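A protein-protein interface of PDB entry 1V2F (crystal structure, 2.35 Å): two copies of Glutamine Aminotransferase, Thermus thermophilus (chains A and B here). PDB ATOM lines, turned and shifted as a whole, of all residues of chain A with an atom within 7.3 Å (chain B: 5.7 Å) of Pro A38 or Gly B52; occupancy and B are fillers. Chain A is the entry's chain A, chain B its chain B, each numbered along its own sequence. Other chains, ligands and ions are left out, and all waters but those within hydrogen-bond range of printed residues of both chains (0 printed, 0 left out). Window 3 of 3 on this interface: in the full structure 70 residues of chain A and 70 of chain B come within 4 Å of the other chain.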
ATOM      1  N   PRO A  35     -21.450   0.710  17.063  1.00  0.00           N
ATOM      2  CA  PRO A  35     -22.416  -0.348  16.736  1.00  0.00           C
ATOM      3  C   PRO A  35     -22.263  -1.639  17.537  1.00  0.00           C
ATOM      4  O   PRO A  35     -21.150  -2.040  17.861  1.00  0.00           O
ATOM      5  CB  PRO A  35     -22.182  -0.578  15.240  1.00  0.00           C
ATOM      6  CG  PRO A  35     -21.581   0.728  14.764  1.00  0.00           C
ATOM      7  CD  PRO A  35     -20.657   1.086  15.878  1.00  0.00           C
ATOM      8  N   SER A  36     -23.392  -2.276  17.845  1.00  0.00           N
ATOM      9  CA  SER A  36     -23.437  -3.551  18.577  1.00  0.00           C
ATOM     10  C   SER A  36     -23.153  -4.698  17.616  1.00  0.00           C
ATOM     11  O   SER A  36     -22.763  -5.783  18.026  1.00  0.00           O
ATOM     12  CB  SER A  36     -24.830  -3.804  19.170  1.00  0.00           C
ATOM     13  OG  SER A  36     -24.999  -3.158  20.404  1.00  0.00           O
ATOM     14  N   ASN A  37     -23.391  -4.451  16.335  1.00  0.00           N
ATOM     15  CA  ASN A  37     -23.177  -5.449  15.300  1.00  0.00           C
ATOM     16  C   ASN A  37     -21.773  -5.350  14.710  1.00  0.00           C
ATOM     17  O   ASN A  37     -21.064  -4.361  14.916  1.00  0.00           O
ATOM     18  CB  ASN A  37     -24.217  -5.252  14.198  1.00  0.00           C
ATOM     19  CG  ASN A  37     -24.243  -3.824  13.674  1.00  0.00           C
ATOM     20  OD1 ASN A  37     -23.504  -3.464  12.750  1.00  0.00           O
ATOM     21  ND2 ASN A  37     -25.083  -2.996  14.278  1.00  0.00           N
ATOM     22  N   PRO A  38     -21.340  -6.391  13.989  1.00  0.00           N
ATOM     23  CA  PRO A  38     -20.005  -6.349  13.388  1.00  0.00           C
ATOM     24  C   PRO A  38     -20.107  -5.629  12.043  1.00  0.00           C
ATOM     25  O   PRO A  38     -21.207  -5.366  11.562  1.00  0.00           O
ATOM     26  CB  PRO A  38     -19.661  -7.829  13.231  1.00  0.00           C
ATOM     27  CG  PRO A  38     -20.977  -8.437  12.919  1.00  0.00           C
ATOM     28  CD  PRO A  38     -21.917  -7.747  13.892  1.00  0.00           C
ATOM     29  N   PRO A  39     -18.967  -5.275  11.433  1.00  0.00           N
ATOM     30  CA  PRO A  39     -19.074  -4.595  10.141  1.00  0.00           C
ATOM     31  C   PRO A  39     -19.600  -5.535   9.043  1.00  0.00           C
ATOM     32  O   PRO A  39     -19.728  -6.746   9.246  1.00  0.00           O
ATOM     33  CB  PRO A  39     -17.648  -4.106   9.887  1.00  0.00           C
ATOM     34  CG  PRO A  39     -16.801  -5.044  10.664  1.00  0.00           C
ATOM     35  CD  PRO A  39     -17.576  -5.287  11.918  1.00  0.00           C
ATOM     36  N   PRO A  40     -19.942  -4.983   7.874  1.00  0.00           N
ATOM     37  CA  PRO A  40     -20.451  -5.835   6.791  1.00  0.00           C
ATOM     38  C   PRO A  40     -19.418  -6.853   6.291  1.00  0.00           C
ATOM     39  O   PRO A  40     -18.215  -6.599   6.300  1.00  0.00           O
ATOM     40  CB  PRO A  40     -20.860  -4.825   5.724  1.00  0.00           C
ATOM     41  CG  PRO A  40     -19.872  -3.707   5.940  1.00  0.00           C
ATOM     42  CD  PRO A  40     -19.867  -3.575   7.449  1.00  0.00           C
ATOM     43  N   PRO A  41     -19.886  -8.028   5.854  1.00  0.00           N
ATOM     44  CA  PRO A  41     -19.005  -9.087   5.355  1.00  0.00           C
ATOM     45  C   PRO A  41     -18.036  -8.668   4.244  1.00  0.00           C
ATOM     46  O   PRO A  41     -16.892  -9.122   4.228  1.00  0.00           O
ATOM     47  CB  PRO A  41     -19.989 -10.166   4.893  1.00  0.00           C
ATOM     48  CG  PRO A  41     -21.161  -9.975   5.816  1.00  0.00           C
ATOM     49  CD  PRO A  41     -21.297  -8.468   5.831  1.00  0.00           C
ATOM     50  N   LEU A  44     -15.010  -7.232   5.951  1.00  0.00           N
ATOM     51  CA  LEU A  44     -14.232  -8.248   6.640  1.00  0.00           C
ATOM     52  C   LEU A  44     -13.438  -9.073   5.628  1.00  0.00           C
ATOM     53  O   LEU A  44     -12.244  -9.294   5.822  1.00  0.00           O
ATOM     54  CB  LEU A  44     -15.134  -9.166   7.475  1.00  0.00           C
ATOM     55  CG  LEU A  44     -15.976  -8.489   8.565  1.00  0.00           C
ATOM     56  CD1 LEU A  44     -16.781  -9.542   9.320  1.00  0.00           C
ATOM     57  CD2 LEU A  44     -15.075  -7.711   9.521  1.00  0.00           C
ATOM     58  N   ARG A  48      -9.339  -9.592   5.264  1.00  0.00           N
ATOM     59  CA  ARG A  48      -8.713 -10.923   5.301  1.00  0.00           C
ATOM     60  C   ARG A  48      -7.776 -11.095   4.112  1.00  0.00           C
ATOM     61  O   ARG A  48      -6.682 -11.640   4.228  1.00  0.00           O
ATOM     62  CB  ARG A  48      -9.767 -12.021   5.220  1.00  0.00           C
ATOM     63  CG  ARG A  48     -10.414 -12.350   6.524  1.00  0.00           C
ATOM     64  CD  ARG A  48     -11.552 -13.340   6.325  1.00  0.00           C
ATOM     65  NE  ARG A  48     -12.081 -13.734   7.620  1.00  0.00           N
ATOM     66  CZ  ARG A  48     -11.524 -14.657   8.390  1.00  0.00           C
ATOM     67  NH1 ARG A  48     -10.431 -15.294   7.977  1.00  0.00           N
ATOM     68  NH2 ARG A  48     -12.032 -14.907   9.588  1.00  0.00           N
ATOM     69  N   LEU A 224     -18.559   2.530   7.736  1.00  0.00           N
ATOM     70  CA  LEU A 224     -18.750   1.085   7.652  1.00  0.00           C
ATOM     71  C   LEU A 224     -18.914   0.254   8.938  1.00  0.00           C
ATOM     72  O   LEU A 224     -18.525  -0.914   8.967  1.00  0.00           O
ATOM     73  CB  LEU A 224     -17.590   0.524   6.819  1.00  0.00           C
ATOM     74  CG  LEU A 224     -17.340   1.220   5.466  1.00  0.00           C
ATOM     75  CD1 LEU A 224     -15.985   0.829   4.907  1.00  0.00           C
ATOM     76  CD2 LEU A 224     -18.435   0.851   4.487  1.00  0.00           C
ATOM     77  N   GLU A 225     -19.478   0.838   9.993  1.00  0.00           N
ATOM     78  CA  GLU A 225     -19.705   0.108  11.243  1.00  0.00           C
ATOM     79  C   GLU A 225     -18.444  -0.578  11.786  1.00  0.00           C
ATOM     80  O   GLU A 225     -18.494  -1.727  12.212  1.00  0.00           O
ATOM     81  CB  GLU A 225     -20.791  -0.959  11.024  1.00  0.00           C
ATOM     82  CG  GLU A 225     -22.080  -0.455  10.363  1.00  0.00           C
ATOM     83  CD  GLU A 225     -23.081   0.115  11.358  1.00  0.00           C
ATOM     84  OE1 GLU A 225     -23.679  -0.670  12.110  1.00  0.00           O
ATOM     85  OE2 GLU A 225     -23.272   1.344  11.390  1.00  0.00           O
ATOM     86  N   ALA A 226     -17.314   0.119  11.780  1.00  0.00           N
ATOM     87  CA  ALA A 226     -16.067  -0.470  12.259  1.00  0.00           C
ATOM     88  C   ALA A 226     -15.224   0.615  12.931  1.00  0.00           C
ATOM     89  O   ALA A 226     -14.125   0.928  12.473  1.00  0.00           O
ATOM     90  CB  ALA A 226     -15.309  -1.076  11.081  1.00  0.00           C
ATOM     91  N   TYR A 229     -11.183   0.497  13.556  1.00  0.00           N
ATOM     92  CA  TYR A 229     -10.175   0.298  12.513  1.00  0.00           C
ATOM     93  C   TYR A 229      -9.190   1.462  12.415  1.00  0.00           C
ATOM     94  O   TYR A 229      -8.080   1.295  11.926  1.00  0.00           O
ATOM     95  CB  TYR A 229     -10.854   0.027  11.153  1.00  0.00           C
ATOM     96  CG  TYR A 229     -11.402  -1.385  11.020  1.00  0.00           C
ATOM     97  CD1 TYR A 229     -11.569  -2.196  12.145  1.00  0.00           C
ATOM     98  CD2 TYR A 229     -11.775  -1.904   9.774  1.00  0.00           C
ATOM     99  CE1 TYR A 229     -12.090  -3.477  12.044  1.00  0.00           C
ATOM    100  CE2 TYR A 229     -12.300  -3.194   9.658  1.00  0.00           C
ATOM    101  CZ  TYR A 229     -12.455  -3.973  10.800  1.00  0.00           C
ATOM    102  OH  TYR A 229     -12.983  -5.239  10.719  1.00  0.00           O
ATOM    103  N   ALA B  50     -10.143 -12.431  15.249  1.00  0.00           N
ATOM    104  CA  ALA B  50     -10.688 -11.217  15.844  1.00  0.00           C
ATOM    105  C   ALA B  50     -11.602 -10.457  14.887  1.00  0.00           C
ATOM    106  O   ALA B  50     -12.512  -9.757  15.325  1.00  0.00           O
ATOM    107  CB  ALA B  50      -9.546 -10.298  16.315  1.00  0.00           C
ATOM    108  N   LEU B  51     -11.362 -10.587  13.584  1.00  0.00           N
ATOM    109  CA  LEU B  51     -12.189  -9.892  12.602  1.00  0.00           C
ATOM    110  C   LEU B  51     -13.637 -10.325  12.733  1.00  0.00           C
ATOM    111  O   LEU B  51     -13.937 -11.512  12.690  1.00  0.00           O
ATOM    112  CB  LEU B  51     -11.688 -10.172  11.191  1.00  0.00           C
ATOM    113  CG  LEU B  51     -10.373  -9.476  10.850  1.00  0.00           C
ATOM    114  CD1 LEU B  51      -9.914  -9.916   9.465  1.00  0.00           C
ATOM    115  CD2 LEU B  51     -10.565  -7.955  10.916  1.00  0.00           C
ATOM    116  N   GLY B  52     -14.532  -9.357  12.891  1.00  0.00           N
ATOM    117  CA  GLY B  52     -15.939  -9.666  13.049  1.00  0.00           C
ATOM    118  C   GLY B  52     -16.365  -9.789  14.510  1.00  0.00           C
ATOM    119  O   GLY B  52     -17.555  -9.786  14.819  1.00  0.00           O
ATOM    120  N   ARG B  53     -15.394  -9.886  15.414  1.00  0.00           N
ATOM    121  CA  ARG B  53     -15.683 -10.024  16.842  1.00  0.00           C
ATOM    122  C   ARG B  53     -15.256  -8.802  17.636  1.00  0.00           C
ATOM    123  O   ARG B  53     -15.978  -8.335  18.516  1.00  0.00           O
ATOM    124  CB  ARG B  53     -14.968 -11.247  17.412  1.00  0.00           C
ATOM    125  CG  ARG B  53     -15.576 -12.584  17.031  1.00  0.00           C
ATOM    126  CD  ARG B  53     -14.754 -13.698  17.666  1.00  0.00           C
ATOM    127  NE  ARG B  53     -14.397 -13.379  19.054  1.00  0.00           N
ATOM    128  CZ  ARG B  53     -13.149 -13.271  19.512  1.00  0.00           C
ATOM    129  NH1 ARG B  53     -12.113 -13.461  18.699  1.00  0.00           N
ATOM    130  NH2 ARG B  53     -12.938 -12.949  20.787  1.00  0.00           N
ATOM    131  N   GLN B  54     -14.068  -8.295  17.326  1.00  0.00           N
ATOM    132  CA  GLN B  54     -13.533  -7.132  18.006  1.00  0.00           C
ATOM    133  C   GLN B  54     -13.167  -6.054  16.999  1.00  0.00           C
ATOM    134  O   GLN B  54     -11.999  -5.854  16.688  1.00  0.00           O
ATOM    135  CB  GLN B  54     -12.322  -7.555  18.830  1.00  0.00           C
ATOM    136  CG  GLN B  54     -12.727  -8.416  20.012  1.00  0.00           C
ATOM    137  CD  GLN B  54     -11.565  -8.814  20.877  1.00  0.00           C
ATOM    138  OE1 GLN B  54     -10.816  -9.730  20.546  1.00  0.00           O
ATOM    139  NE2 GLN B  54     -11.397  -8.120  21.995  1.00  0.00           N
ATOM    140  N   ASP B  55     -14.179  -5.347  16.507  1.00  0.00           N
ATOM    141  CA  ASP B  55     -13.972  -4.313  15.503  1.00  0.00           C
ATOM    142  C   ASP B  55     -14.262  -2.887  15.972  1.00  0.00           C
ATOM    143  O   ASP B  55     -13.904  -1.931  15.295  1.00  0.00           O
ATOM    144  CB  ASP B  55     -14.842  -4.618  14.278  1.00  0.00           C
ATOM    145  CG  ASP B  55     -14.679  -6.053  13.783  1.00  0.00           C
ATOM    146  OD1 ASP B  55     -13.699  -6.353  13.067  1.00  0.00           O
ATOM    147  OD2 ASP B  55     -15.534  -6.886  14.126  1.00  0.00           O
ATOM    148  N   GLN B  56     -14.901  -2.740  17.126  1.00  0.00           N
ATOM    149  CA  GLN B  56     -15.252  -1.413  17.612  1.00  0.00           C
ATOM    150  C   GLN B  56     -14.203  -0.800  18.546  1.00  0.00           C
ATOM    151  O   GLN B  56     -13.213  -1.443  18.883  1.00  0.00           O
ATOM    152  CB  GLN B  56     -16.618  -1.463  18.307  1.00  0.00           C
ATOM    153  CG  GLN B  56     -17.725  -2.145  17.496  1.00  0.00           C
ATOM    154  CD  GLN B  56     -17.832  -1.640  16.058  1.00  0.00           C
ATOM    155  OE1 GLN B  56     -17.667  -0.443  15.780  1.00  0.00           O
ATOM    156  NE2 GLN B  56     -18.127  -2.553  15.136  1.00  0.00           N
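No position is printed for both chains.
OE1 of Glu A225 sits close to OD1 of Asn A37.
The backbone NH (N) of Gly B52 is in hydrogen-bond range of the side-chain carboxylate (OD2) of Asp B55, 2.9 Å away.
The backbone NH of Arg B53 is in hydrogen-bond range of the side-chain carboxylate of Asp B55.
Pro A38 touches just one residue of chain B: Gly B52.
Gly B52 touches just these residues of chain A: Pro A38 (3.3 Å) and Leu A44 (3.8 Å).
Of the printed residues of chain B, Tyr A229 touches Leu B51 and Asp B55.
Of the printed residues of chain B, Ala A226 touches Asp B55 and Gln B56.
Of the printed residues of chain B, Pro A39 touches Asp B55.
Printed residues of chain B within 4 Å of Pro A35: Gln B56 (3.4 Å).
Printed residues of chain B within 4 Å of Leu A44: Gly B52.
Among the printed residues, merely in contact across the chains: Pro A38 with Gly B52 (3.3 Å), Pro A35 with Gln B56 (3.4 Å), Pro A39 with Asp B55 (3.4 Å), Tyr A229 with Leu B51 (3.6 Å), Ala A226 with Asp B55 (3.7 Å), Leu A44 with Gly B52 (3.8 Å), Arg A48 with Leu B51 (3.9 Å) and Ala A226 with Gln B56 (3.9 Å).
Of the 7 printed residues of chain B, 4 touch a printed residue of chain A.
Printed residues of chain B that touch a printed residue of chain A: Leu B51, Gly B52, Asp B55 and Gln B56.
Printed residues of chain A that touch a printed residue of chain B: Pro A35, Asn A37, Pro A38, Pro A39, Leu A44, Arg A48, Glu A225, Ala A226 and Tyr A229.
Among the printed residues, 11 pairs touch across the chains.
Among the printed residues, no Asp or Glu carboxylate lies within 4 Å of a Lys or Arg side-chain nitrogen of the other chain.
OH of Tyr A229 lies within hydrogen-bond range of OD1 of Asp B55.
The side-chain amide nitrogen (NE2) of Gln B56 lies within hydrogen-bond range of the backbone carbonyl oxygen (O) of Asn A37.
The backbone carbonyl oxygen (O) of Glu A225 is in hydrogen-bond range of the side-chain amide nitrogen (NE2) of Gln B56, 3.1 Å away.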
